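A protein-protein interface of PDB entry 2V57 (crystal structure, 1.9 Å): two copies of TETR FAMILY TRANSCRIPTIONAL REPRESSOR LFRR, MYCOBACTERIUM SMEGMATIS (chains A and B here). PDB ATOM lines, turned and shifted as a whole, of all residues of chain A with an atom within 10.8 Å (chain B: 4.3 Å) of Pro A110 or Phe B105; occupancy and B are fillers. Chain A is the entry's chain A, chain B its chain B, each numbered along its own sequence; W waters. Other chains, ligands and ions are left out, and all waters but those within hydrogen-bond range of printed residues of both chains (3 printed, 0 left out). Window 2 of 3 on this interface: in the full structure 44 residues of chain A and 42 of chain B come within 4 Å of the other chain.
Leu B104 touches Tyr A108 (O to CE1, 3.5 Å). CD2 of Tyr B107 touches OH of Tyr A108, at 3.7 Å. Pro A110 touches Pro B31. Pro A110 touches Phe B105. Ser A111 touches Thr B32.
Of the 24 printed residues of chain A, 3 touch a printed residue of chain B. Printed residues of chain A that touch a printed residue of chain B: Tyr A108, Pro A110 and Ser A111. Hydrophobic or aromatic side chains of chain A within 4 Å of the printed part of chain B: Tyr A108 and Pro A110. Of the 12 printed residues of chain B, 5 touch a printed residue of chain A. Printed residues of chain B that touch a printed residue of chain A: Pro B31, Thr B32, Leu B104, Phe B105 and Tyr B107. Hydrophobic or aromatic side chains of chain B that line the printed part of chain A: Pro B31, Phe B105 and Tyr B107. Along chain B the printed residues that touch a printed residue of chain A span positions 31 to 107. Among the printed residues, no Asp or Glu carboxylate lies within 4 Å of a Lys or Arg side-chain nitrogen of the other chain.
The side-chain carboxylate of Glu A109 sits at hydrogen-bond distance from the side-chain hydroxyl of Ser A111, 2.5 Å away. NE2 of Gln A157 sits at hydrogen-bond distance from OH of Tyr A108 (3.1 Å). The backbone carbonyl oxygen (O) of Ser A111 lies within hydrogen-bond range of the guanidinium group (NH2) of Arg A61.
Water W1 lies within hydrogen-bond range of the backbone carbonyl oxygen (O) of Tyr A108 (2.9 Å) and the backbone carbonyl oxygen (O) of Leu B104 (3.5 Å). Water W3 bridges the backbone carbonyl oxygen of Tyr A108 and the backbone carbonyl oxygen of Phe B105. Water W2 bridges OE1 of Gln A157 (3.0 Å) and OH of Tyr B107 (3.2 Å).
Pro A110 touches just these residues of chain B: Pro B31 (3.9 Å) and Phe B105 (3.9 Å). Phe B105 touches just one residue of chain A: Pro A110. No residue of chain A comes within 4 Å of Leu B27. Leu B60 touches none of the printed residues of chain A. No residue of chain A comes within 4 Å of Ile B102. Leu B104 touches just one residue of chain A: Tyr A108 (3.5 Å). No residue of chain A comes within 4 Å of Val B106. Of the printed residues of chain A, Tyr B107 touches Tyr A108 (3.7 Å). Of the printed residues of chain B, Ser A111 touches Thr B32 (3.8 Å). Ala A119 touches none of the printed residues of chain B. Tyr A107 touches none of the printed residues of chain B. The nearest residue of chain A that does not touch Phe B105 is Tyr A108 (5.2 Å). The nearest printed residue of chain B that does not touch Ser A111 is Pro B31 (5.5 Å).
9 positions are printed for both chains.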
ATOM      1  N   PRO A  31     -17.429 -25.160   8.841  1.00  0.00           N
ATOM      2  CA  PRO A  31     -17.167 -23.988   9.687  1.00  0.00           C
ATOM      3  C   PRO A  31     -17.822 -24.040  11.053  1.00  0.00           C
ATOM      4  O   PRO A  31     -17.452 -23.244  11.912  1.00  0.00           O
ATOM      5  CB  PRO A  31     -17.746 -22.818   8.879  1.00  0.00           C
ATOM      6  CG  PRO A  31     -17.836 -23.340   7.458  1.00  0.00           C
ATOM      7  CD  PRO A  31     -18.121 -24.811   7.592  1.00  0.00           C
ATOM      8  N   THR A  32     -18.794 -24.926  11.249  1.00  0.00           N
ATOM      9  CA  THR A  32     -19.423 -25.038  12.548  1.00  0.00           C
ATOM     10  C   THR A  32     -18.965 -26.299  13.272  1.00  0.00           C
ATOM     11  O   THR A  32     -19.562 -26.676  14.280  1.00  0.00           O
ATOM     12  CB  THR A  32     -20.969 -25.050  12.445  1.00  0.00           C
ATOM     13  OG1 THR A  32     -21.399 -26.224  11.746  1.00  0.00           O
ATOM     14  CG2 THR A  32     -21.481 -23.800  11.720  1.00  0.00           C
ATOM     15  N   ARG A  56     -13.297 -21.367  22.279  1.00  0.00           N
ATOM     16  CA  ARG A  56     -13.324 -21.500  20.831  1.00  0.00           C
ATOM     17  C   ARG A  56     -12.716 -20.268  20.188  1.00  0.00           C
ATOM     18  O   ARG A  56     -11.999 -20.355  19.189  1.00  0.00           O
ATOM     19  CB  ARG A  56     -14.756 -21.694  20.326  1.00  0.00           C
ATOM     20  CG  ARG A  56     -14.843 -21.954  18.819  1.00  0.00           C
ATOM     21  CD  ARG A  56     -16.293 -22.024  18.330  1.00  0.00           C
ATOM     22  NE  ARG A  56     -16.389 -22.387  16.916  1.00  0.00           N
ATOM     23  CZ  ARG A  56     -16.430 -23.642  16.479  1.00  0.00           C
ATOM     24  NH1 ARG A  56     -16.380 -24.640  17.351  1.00  0.00           N
ATOM     25  NH2 ARG A  56     -16.518 -23.902  15.177  1.00  0.00           N
ATOM     26  N   THR A  57     -13.012 -19.111  20.766  1.00  0.00           N
ATOM     27  CA  THR A  57     -12.493 -17.872  20.226  1.00  0.00           C
ATOM     28  C   THR A  57     -10.965 -17.872  20.264  1.00  0.00           C
ATOM     29  O   THR A  57     -10.324 -17.420  19.321  1.00  0.00           O
ATOM     30  CB  THR A  57     -13.077 -16.639  20.964  1.00  0.00           C
ATOM     31  OG1 THR A  57     -14.467 -16.507  20.630  1.00  0.00           O
ATOM     32  CG2 THR A  57     -12.349 -15.377  20.548  1.00  0.00           C
ATOM     33  N   LEU A  60      -9.823 -19.916  17.354  1.00  0.00           N
ATOM     34  CA  LEU A  60     -10.085 -19.254  16.075  1.00  0.00           C
ATOM     35  C   LEU A  60      -9.087 -18.123  15.788  1.00  0.00           C
ATOM     36  O   LEU A  60      -8.664 -17.934  14.636  1.00  0.00           O
ATOM     37  CB  LEU A  60     -11.525 -18.728  16.016  1.00  0.00           C
ATOM     38  CG  LEU A  60     -12.652 -19.758  15.990  1.00  0.00           C
ATOM     39  CD1 LEU A  60     -13.994 -19.073  15.682  1.00  0.00           C
ATOM     40  CD2 LEU A  60     -12.372 -20.888  14.991  1.00  0.00           C
ATOM     41  N   ARG A  61      -8.731 -17.364  16.824  1.00  0.00           N
ATOM     42  CA  ARG A  61      -7.768 -16.273  16.667  1.00  0.00           C
ATOM     43  C   ARG A  61      -6.333 -16.770  16.471  1.00  0.00           C
ATOM     44  O   ARG A  61      -5.583 -16.205  15.680  1.00  0.00           O
ATOM     45  CB  ARG A  61      -7.886 -15.267  17.812  1.00  0.00           C
ATOM     46  CG  ARG A  61      -9.197 -14.483  17.732  1.00  0.00           C
ATOM     47  CD  ARG A  61      -9.429 -13.564  18.912  1.00  0.00           C
ATOM     48  NE  ARG A  61     -10.704 -12.864  18.766  1.00  0.00           N
ATOM     49  CZ  ARG A  61     -11.330 -12.244  19.759  1.00  0.00           C
ATOM     50  NH1 ARG A  61     -10.781 -12.241  20.967  1.00  0.00           N
ATOM     51  NH2 ARG A  61     -12.500 -11.631  19.545  1.00  0.00           N
ATOM     52  N   ALA A  64      -6.291 -17.906  12.914  1.00  0.00           N
ATOM     53  CA  ALA A  64      -6.203 -16.794  11.985  1.00  0.00           C
ATOM     54  C   ALA A  64      -4.769 -16.327  11.886  1.00  0.00           C
ATOM     55  O   ALA A  64      -4.259 -16.085  10.791  1.00  0.00           O
ATOM     56  CB  ALA A  64      -7.093 -15.654  12.435  1.00  0.00           C
ATOM     57  N   VAL A 103      -9.118 -19.327   4.151  1.00  0.00           N
ATOM     58  CA  VAL A 103      -8.888 -17.894   4.096  1.00  0.00           C
ATOM     59  C   VAL A 103     -10.224 -17.150   4.138  1.00  0.00           C
ATOM     60  O   VAL A 103     -10.382 -16.169   4.861  1.00  0.00           O
ATOM     61  CB  VAL A 103      -8.051 -17.499   2.845  1.00  0.00           C
ATOM     62  CG1 VAL A 103      -7.936 -15.971   2.730  1.00  0.00           C
ATOM     63  CG2 VAL A 103      -6.674 -18.157   2.904  1.00  0.00           C
ATOM     64  N   LEU A 104     -11.204 -17.630   3.380  1.00  0.00           N
ATOM     65  CA  LEU A 104     -12.531 -17.036   3.453  1.00  0.00           C
ATOM     66  C   LEU A 104     -13.068 -17.119   4.881  1.00  0.00           C
ATOM     67  O   LEU A 104     -13.638 -16.165   5.403  1.00  0.00           O
ATOM     68  CB  LEU A 104     -13.499 -17.724   2.480  1.00  0.00           C
ATOM     69  CG  LEU A 104     -13.141 -17.647   0.995  1.00  0.00           C
ATOM     70  CD1 LEU A 104     -14.069 -18.562   0.214  1.00  0.00           C
ATOM     71  CD2 LEU A 104     -13.241 -16.220   0.496  1.00  0.00           C
ATOM     72  N   PHE A 105     -12.904 -18.276   5.507  1.00  0.00           N
ATOM     73  CA  PHE A 105     -13.365 -18.442   6.880  1.00  0.00           C
ATOM     74  C   PHE A 105     -12.751 -17.390   7.814  1.00  0.00           C
ATOM     75  O   PHE A 105     -13.470 -16.710   8.570  1.00  0.00           O
ATOM     76  CB  PHE A 105     -13.028 -19.833   7.389  1.00  0.00           C
ATOM     77  CG  PHE A 105     -13.467 -20.078   8.820  1.00  0.00           C
ATOM     78  CD1 PHE A 105     -14.767 -20.453   9.100  1.00  0.00           C
ATOM     79  CD2 PHE A 105     -12.572 -19.945   9.866  1.00  0.00           C
ATOM     80  CE1 PHE A 105     -15.173 -20.685  10.400  1.00  0.00           C
ATOM     81  CE2 PHE A 105     -12.977 -20.184  11.182  1.00  0.00           C
ATOM     82  CZ  PHE A 105     -14.277 -20.551  11.440  1.00  0.00           C
ATOM     83  N   VAL A 106     -11.428 -17.243   7.764  1.00  0.00           N
ATOM     84  CA  VAL A 106     -10.751 -16.331   8.681  1.00  0.00           C
ATOM     85  C   VAL A 106     -11.199 -14.873   8.517  1.00  0.00           C
ATOM     86  O   VAL A 106     -11.347 -14.135   9.498  1.00  0.00           O
ATOM     87  CB  VAL A 106      -9.212 -16.425   8.508  1.00  0.00           C
ATOM     88  CG1 VAL A 106      -8.543 -15.166   9.013  1.00  0.00           C
ATOM     89  CG2 VAL A 106      -8.689 -17.679   9.204  1.00  0.00           C
ATOM     90  N   TYR A 107     -11.393 -14.447   7.272  1.00  0.00           N
ATOM     91  CA  TYR A 107     -11.819 -13.077   7.029  1.00  0.00           C
ATOM     92  C   TYR A 107     -13.297 -12.824   7.316  1.00  0.00           C
ATOM     93  O   TYR A 107     -13.684 -11.697   7.616  1.00  0.00           O
ATOM     94  CB  TYR A 107     -11.454 -12.649   5.596  1.00  0.00           C
ATOM     95  CG  TYR A 107     -10.006 -12.272   5.476  1.00  0.00           C
ATOM     96  CD1 TYR A 107      -9.590 -10.952   5.659  1.00  0.00           C
ATOM     97  CD2 TYR A 107      -9.037 -13.237   5.211  1.00  0.00           C
ATOM     98  CE1 TYR A 107      -8.245 -10.607   5.575  1.00  0.00           C
ATOM     99  CE2 TYR A 107      -7.688 -12.895   5.129  1.00  0.00           C
ATOM    100  CZ  TYR A 107      -7.304 -11.582   5.303  1.00  0.00           C
ATOM    101  OH  TYR A 107      -5.960 -11.257   5.210  1.00  0.00           O
ATOM    102  N   TYR A 108     -14.126 -13.863   7.252  1.00  0.00           N
ATOM    103  CA  TYR A 108     -15.563 -13.655   7.413  1.00  0.00           C
ATOM    104  C   TYR A 108     -16.189 -14.047   8.770  1.00  0.00           C
ATOM    105  O   TYR A 108     -17.293 -13.586   9.111  1.00  0.00           O
ATOM    106  CB  TYR A 108     -16.318 -14.278   6.247  1.00  0.00           C
ATOM    107  CG  TYR A 108     -16.321 -13.405   5.017  1.00  0.00           C
ATOM    108  CD1 TYR A 108     -17.020 -12.199   5.009  1.00  0.00           C
ATOM    109  CD2 TYR A 108     -15.664 -13.786   3.857  1.00  0.00           C
ATOM    110  CE1 TYR A 108     -17.053 -11.389   3.876  1.00  0.00           C
ATOM    111  CE2 TYR A 108     -15.674 -12.980   2.720  1.00  0.00           C
ATOM    112  CZ  TYR A 108     -16.381 -11.779   2.737  1.00  0.00           C
ATOM    113  OH  TYR A 108     -16.422 -10.960   1.622  1.00  0.00           O
ATOM    114  N   GLU A 109     -15.487 -14.857   9.555  1.00  0.00           N
ATOM    115  CA  GLU A 109     -15.996 -15.245  10.868  1.00  0.00           C
ATOM    116  C   GLU A 109     -15.899 -14.024  11.776  1.00  0.00           C
ATOM    117  O   GLU A 109     -14.804 -13.528  12.042  1.00  0.00           O
ATOM    118  CB  GLU A 109     -15.201 -16.425  11.439  1.00  0.00           C
ATOM    119  CG  GLU A 109     -16.020 -17.342  12.354  1.00  0.00           C
ATOM    120  CD  GLU A 109     -16.355 -16.696  13.694  1.00  0.00           C
ATOM    121  OE1 GLU A 109     -15.584 -15.819  14.142  1.00  0.00           O
ATOM    122  OE2 GLU A 109     -17.383 -17.064  14.305  1.00  0.00           O
ATOM    123  N   PRO A 110     -17.046 -13.517  12.240  1.00  0.00           N
ATOM    124  CA  PRO A 110     -17.106 -12.195  12.878  1.00  0.00           C
ATOM    125  C   PRO A 110     -16.233 -12.037  14.130  1.00  0.00           C
ATOM    126  O   PRO A 110     -15.758 -10.930  14.392  1.00  0.00           O
ATOM    127  CB  PRO A 110     -18.583 -12.056  13.261  1.00  0.00           C
ATOM    128  CG  PRO A 110     -19.312 -12.956  12.310  1.00  0.00           C
ATOM    129  CD  PRO A 110     -18.380 -14.119  12.067  1.00  0.00           C
ATOM    130  N   SER A 111     -16.033 -13.110  14.892  1.00  0.00           N
ATOM    131  CA  SER A 111     -15.342 -12.990  16.163  1.00  0.00           C
ATOM    132  C   SER A 111     -13.830 -12.960  15.982  1.00  0.00           C
ATOM    133  O   SER A 111     -13.088 -12.727  16.940  1.00  0.00           O
ATOM    134  CB  SER A 111     -15.710 -14.156  17.080  1.00  0.00           C
ATOM    135  OG  SER A 111     -15.125 -15.354  16.599  1.00  0.00           O
ATOM    136  N   ILE A 112     -13.368 -13.228  14.765  1.00  0.00           N
ATOM    137  CA  ILE A 112     -11.938 -13.313  14.530  1.00  0.00           C
ATOM    138  C   ILE A 112     -11.263 -11.945  14.393  1.00  0.00           C
ATOM    139  O   ILE A 112     -10.468 -11.558  15.244  1.00  0.00           O
ATOM    140  CB  ILE A 112     -11.610 -14.191  13.313  1.00  0.00           C
ATOM    141  CG1 ILE A 112     -12.040 -15.637  13.596  1.00  0.00           C
ATOM    142  CG2 ILE A 112     -10.120 -14.093  12.993  1.00  0.00           C
ATOM    143  CD1 ILE A 112     -11.635 -16.666  12.516  1.00  0.00           C
ATOM    144  N   LEU A 113     -11.569 -11.216  13.326  1.00  0.00           N
ATOM    145  CA  LEU A 113     -10.899  -9.948  13.101  1.00  0.00           C
ATOM    146  C   LEU A 113     -11.508  -8.818  13.936  1.00  0.00           C
ATOM    147  O   LEU A 113     -11.074  -7.669  13.845  1.00  0.00           O
ATOM    148  CB  LEU A 113     -10.882  -9.593  11.617  1.00  0.00           C
ATOM    149  CG  LEU A 113      -9.898 -10.463  10.852  1.00  0.00           C
ATOM    150  CD1 LEU A 113      -9.942 -10.151   9.371  1.00  0.00           C
ATOM    151  CD2 LEU A 113      -8.491 -10.287  11.406  1.00  0.00           C
ATOM    152  N   ALA A 114     -12.509  -9.159  14.748  1.00  0.00           N
ATOM    153  CA  ALA A 114     -13.070  -8.213  15.708  1.00  0.00           C
ATOM    154  C   ALA A 114     -12.018  -7.803  16.740  1.00  0.00           C
ATOM    155  O   ALA A 114     -12.140  -6.762  17.377  1.00  0.00           O
ATOM    156  CB  ALA A 114     -14.295  -8.802  16.393  1.00  0.00           C
ATOM    157  N   ASP A 115     -10.990  -8.630  16.912  1.00  0.00           N
ATOM    158  CA  ASP A 115      -9.866  -8.284  17.784  1.00  0.00           C
ATOM    159  C   ASP A 115      -8.921  -7.286  17.097  1.00  0.00           C
ATOM    160  O   ASP A 115      -8.272  -7.622  16.100  1.00  0.00           O
ATOM    161  CB  ASP A 115      -9.107  -9.550  18.186  1.00  0.00           C
ATOM    162  CG  ASP A 115      -7.767  -9.256  18.837  1.00  0.00           C
ATOM    163  OD1 ASP A 115      -7.463  -9.876  19.872  1.00  0.00           O
ATOM    164  OD2 ASP A 115      -7.006  -8.422  18.320  1.00  0.00           O
ATOM    165  N   PRO A 116      -8.827  -6.061  17.638  1.00  0.00           N
ATOM    166  CA  PRO A 116      -8.048  -4.973  17.025  1.00  0.00           C
ATOM    167  C   PRO A 116      -6.573  -5.305  16.865  1.00  0.00           C
ATOM    168  O   PRO A 116      -5.971  -4.940  15.854  1.00  0.00           O
ATOM    169  CB  PRO A 116      -8.229  -3.806  18.006  1.00  0.00           C
ATOM    170  CG  PRO A 116      -9.513  -4.108  18.713  1.00  0.00           C
ATOM    171  CD  PRO A 116      -9.547  -5.613  18.841  1.00  0.00           C
ATOM    172  N   LEU A 118      -5.219  -8.344  16.413  1.00  0.00           N
ATOM    173  CA  LEU A 118      -5.111  -9.293  15.311  1.00  0.00           C
ATOM    174  C   LEU A 118      -5.383  -8.591  13.977  1.00  0.00           C
ATOM    175  O   LEU A 118      -4.735  -8.874  12.970  1.00  0.00           O
ATOM    176  CB  LEU A 118      -6.099 -10.436  15.528  1.00  0.00           C
ATOM    177  CG  LEU A 118      -5.997 -11.646  14.597  1.00  0.00           C
ATOM    178  CD1 LEU A 118      -4.622 -12.213  14.650  1.00  0.00           C
ATOM    179  CD2 LEU A 118      -7.006 -12.684  15.009  1.00  0.00           C
ATOM    180  N   ALA A 119      -6.338  -7.668  13.969  1.00  0.00           N
ATOM    181  CA  ALA A 119      -6.656  -6.938  12.746  1.00  0.00           C
ATOM    182  C   ALA A 119      -5.442  -6.147  12.266  1.00  0.00           C
ATOM    183  O   ALA A 119      -5.187  -6.041  11.061  1.00  0.00           O
ATOM    184  CB  ALA A 119      -7.833  -6.014  12.974  1.00  0.00           C
ATOM    185  N   GLN A 157     -10.113 -13.110  -3.423  1.00  0.00           N
ATOM    186  CA  GLN A 157     -11.356 -13.598  -2.826  1.00  0.00           C
ATOM    187  C   GLN A 157     -12.272 -14.320  -3.803  1.00  0.00           C
ATOM    188  O   GLN A 157     -12.791 -15.406  -3.496  1.00  0.00           O
ATOM    189  CB  GLN A 157     -12.153 -12.462  -2.177  1.00  0.00           C
ATOM    190  CG  GLN A 157     -13.428 -12.993  -1.577  1.00  0.00           C
ATOM    191  CD  GLN A 157     -14.318 -11.917  -1.003  1.00  0.00           C
ATOM    192  OE1 GLN A 157     -15.446 -11.711  -1.455  1.00  0.00           O
ATOM    193  NE2 GLN A 157     -13.819 -11.233  -0.002  1.00  0.00           N
ATOM    194  N   LEU B  27     -24.338  -4.397  14.301  1.00  0.00           N
ATOM    195  CA  LEU B  27     -23.412  -5.458  13.909  1.00  0.00           C
ATOM    196  C   LEU B  27     -22.385  -4.981  12.896  1.00  0.00           C
ATOM    197  O   LEU B  27     -21.321  -5.574  12.775  1.00  0.00           O
ATOM    198  CB  LEU B  27     -24.174  -6.678  13.369  1.00  0.00           C
ATOM    199  CG  LEU B  27     -25.060  -7.370  14.401  1.00  0.00           C
ATOM    200  CD1 LEU B  27     -26.004  -8.337  13.700  1.00  0.00           C
ATOM    201  CD2 LEU B  27     -24.199  -8.086  15.443  1.00  0.00           C
ATOM    202  N   PRO B  31     -19.408  -6.553  15.514  1.00  0.00           N
ATOM    203  CA  PRO B  31     -19.847  -7.846  14.965  1.00  0.00           C
ATOM    204  C   PRO B  31     -20.162  -8.911  16.011  1.00  0.00           C
ATOM    205  O   PRO B  31     -20.909  -9.850  15.712  1.00  0.00           O
ATOM    206  CB  PRO B  31     -18.662  -8.294  14.098  1.00  0.00           C
ATOM    207  CG  PRO B  31     -17.810  -7.068  13.903  1.00  0.00           C
ATOM    208  CD  PRO B  31     -18.033  -6.205  15.110  1.00  0.00           C
ATOM    209  N   THR B  32     -19.620  -8.768  17.211  1.00  0.00           N
ATOM    210  CA  THR B  32     -19.890  -9.731  18.267  1.00  0.00           C
ATOM    211  C   THR B  32     -20.972  -9.277  19.241  1.00  0.00           C
ATOM    212  O   THR B  32     -21.166  -9.920  20.269  1.00  0.00           O
ATOM    213  CB  THR B  32     -18.614 -10.063  19.079  1.00  0.00           C
ATOM    214  OG1 THR B  32     -18.080  -8.868  19.658  1.00  0.00           O
ATOM    215  CG2 THR B  32     -17.559 -10.694  18.187  1.00  0.00           C
ATOM    216  N   LEU B  60     -29.441 -13.456  13.065  1.00  0.00           N
ATOM    217  CA  LEU B  60     -28.414 -13.352  12.035  1.00  0.00           C
ATOM    218  C   LEU B  60     -28.932 -13.830  10.678  1.00  0.00           C
ATOM    219  O   LEU B  60     -28.678 -13.199   9.648  1.00  0.00           O
ATOM    220  CB  LEU B  60     -27.161 -14.144  12.454  1.00  0.00           C
ATOM    221  CG  LEU B  60     -25.991 -13.391  13.106  1.00  0.00           C
ATOM    222  CD1 LEU B  60     -26.426 -12.218  13.981  1.00  0.00           C
ATOM    223  CD2 LEU B  60     -25.048 -14.347  13.874  1.00  0.00           C
ATOM    224  N   PRO B 101     -21.925  -1.205   5.075  1.00  0.00           N
ATOM    225  CA  PRO B 101     -20.985  -2.253   5.470  1.00  0.00           C
ATOM    226  C   PRO B 101     -21.625  -3.482   6.112  1.00  0.00           C
ATOM    227  O   PRO B 101     -20.889  -4.428   6.362  1.00  0.00           O
ATOM    228  CB  PRO B 101     -20.069  -1.532   6.475  1.00  0.00           C
ATOM    229  CG  PRO B 101     -20.907  -0.396   6.984  1.00  0.00           C
ATOM    230  CD  PRO B 101     -21.653   0.064   5.774  1.00  0.00           C
ATOM    231  N   ILE B 102     -22.931  -3.500   6.376  1.00  0.00           N
ATOM    232  CA  ILE B 102     -23.530  -4.732   6.912  1.00  0.00           C
ATOM    233  C   ILE B 102     -23.393  -5.870   5.894  1.00  0.00           C
ATOM    234  O   ILE B 102     -23.384  -7.061   6.238  1.00  0.00           O
ATOM    235  CB  ILE B 102     -25.013  -4.547   7.346  1.00  0.00           C
ATOM    236  CG1 ILE B 102     -25.463  -5.716   8.240  1.00  0.00           C
ATOM    237  CG2 ILE B 102     -25.931  -4.381   6.132  1.00  0.00           C
ATOM    238  CD1 ILE B 102     -24.735  -5.749   9.593  1.00  0.00           C
ATOM    239  N   VAL B 103     -23.257  -5.509   4.625  1.00  0.00           N
ATOM    240  CA  VAL B 103     -23.051  -6.520   3.587  1.00  0.00           C
ATOM    241  C   VAL B 103     -21.792  -7.365   3.835  1.00  0.00           C
ATOM    242  O   VAL B 103     -21.768  -8.544   3.501  1.00  0.00           O
ATOM    243  CB  VAL B 103     -23.053  -5.899   2.163  1.00  0.00           C
ATOM    244  CG1 VAL B 103     -22.782  -6.966   1.102  1.00  0.00           C
ATOM    245  CG2 VAL B 103     -24.384  -5.172   1.915  1.00  0.00           C
ATOM    246  N   LEU B 104     -20.764  -6.774   4.445  1.00  0.00           N
ATOM    247  CA  LEU B 104     -19.565  -7.523   4.812  1.00  0.00           C
ATOM    248  C   LEU B 104     -19.883  -8.560   5.872  1.00  0.00           C
ATOM    249  O   LEU B 104     -19.251  -9.624   5.953  1.00  0.00           O
ATOM    250  CB  LEU B 104     -18.491  -6.585   5.366  1.00  0.00           C
ATOM    251  CG  LEU B 104     -17.911  -5.538   4.413  1.00  0.00           C
ATOM    252  CD1 LEU B 104     -17.209  -4.454   5.217  1.00  0.00           C
ATOM    253  CD2 LEU B 104     -16.949  -6.188   3.420  1.00  0.00           C
ATOM    254  N   PHE B 105     -20.848  -8.235   6.719  1.00  0.00           N
ATOM    255  CA  PHE B 105     -21.218  -9.158   7.786  1.00  0.00           C
ATOM    256  C   PHE B 105     -22.019 -10.329   7.206  1.00  0.00           C
ATOM    257  O   PHE B 105     -21.773 -11.485   7.566  1.00  0.00           O
ATOM    258  CB  PHE B 105     -21.985  -8.414   8.897  1.00  0.00           C
ATOM    259  CG  PHE B 105     -22.309  -9.260  10.122  1.00  0.00           C
ATOM    260  CD1 PHE B 105     -21.483  -9.254  11.229  1.00  0.00           C
ATOM    261  CD2 PHE B 105     -23.481 -10.006  10.179  1.00  0.00           C
ATOM    262  CE1 PHE B 105     -21.793 -10.001  12.369  1.00  0.00           C
ATOM    263  CE2 PHE B 105     -23.794 -10.757  11.313  1.00  0.00           C
ATOM    264  CZ  PHE B 105     -22.941 -10.754  12.408  1.00  0.00           C
ATOM    265  N   VAL B 106     -22.950 -10.053   6.288  1.00  0.00           N
ATOM    266  CA  VAL B 106     -23.858 -11.113   5.837  1.00  0.00           C
ATOM    267  C   VAL B 106     -23.451 -11.871   4.565  1.00  0.00           C
ATOM    268  O   VAL B 106     -23.988 -12.935   4.289  1.00  0.00           O
ATOM    269  CB  VAL B 106     -25.323 -10.620   5.684  1.00  0.00           C
ATOM    270  CG1 VAL B 106     -25.802  -9.968   6.991  1.00  0.00           C
ATOM    271  CG2 VAL B 106     -25.459  -9.660   4.493  1.00  0.00           C
ATOM    272  N   TYR B 107     -22.499 -11.340   3.807  1.00  0.00           N
ATOM    273  CA  TYR B 107     -22.148 -11.938   2.513  1.00  0.00           C
ATOM    274  C   TYR B 107     -21.860 -13.444   2.552  1.00  0.00           C
ATOM    275  O   TYR B 107     -22.441 -14.205   1.785  1.00  0.00           O
ATOM    276  CB  TYR B 107     -20.973 -11.194   1.869  1.00  0.00           C
ATOM    277  CG  TYR B 107     -20.637 -11.714   0.485  1.00  0.00           C
ATOM    278  CD1 TYR B 107     -21.438 -11.403  -0.615  1.00  0.00           C
ATOM    279  CD2 TYR B 107     -19.529 -12.515   0.280  1.00  0.00           C
ATOM    280  CE1 TYR B 107     -21.142 -11.890  -1.879  1.00  0.00           C
ATOM    281  CE2 TYR B 107     -19.218 -12.998  -0.985  1.00  0.00           C
ATOM    282  CZ  TYR B 107     -20.027 -12.682  -2.060  1.00  0.00           C
ATOM    283  OH  TYR B 107     -19.711 -13.167  -3.321  1.00  0.00           O
ATOM    284  N   GLU B 109     -22.285 -15.474   5.130  1.00  0.00           N
ATOM    285  CA  GLU B 109     -23.034 -16.103   6.216  1.00  0.00           C
ATOM    286  C   GLU B 109     -23.633 -17.504   5.959  1.00  0.00           C
ATOM    287  O   GLU B 109     -23.644 -18.335   6.870  1.00  0.00           O
ATOM    288  CB  GLU B 109     -24.126 -15.151   6.714  1.00  0.00           C
ATOM    289  CG  GLU B 109     -24.945 -15.709   7.855  1.00  0.00           C
ATOM    290  CD  GLU B 109     -25.640 -14.623   8.657  1.00  0.00           C
ATOM    291  OE1 GLU B 109     -26.893 -14.558   8.609  1.00  0.00           O
ATOM    292  OE2 GLU B 109     -24.927 -13.835   9.326  1.00  0.00           O
HETATM  293  O   HOH W   1     -17.343 -10.719   8.640  1.00  0.00           O
HETATM  294  O   HOH W   2     -16.789 -12.308  -4.126  1.00  0.00           O
HETATM  295  O   HOH W   3     -20.131 -14.134   8.429  1.00  0.00           O
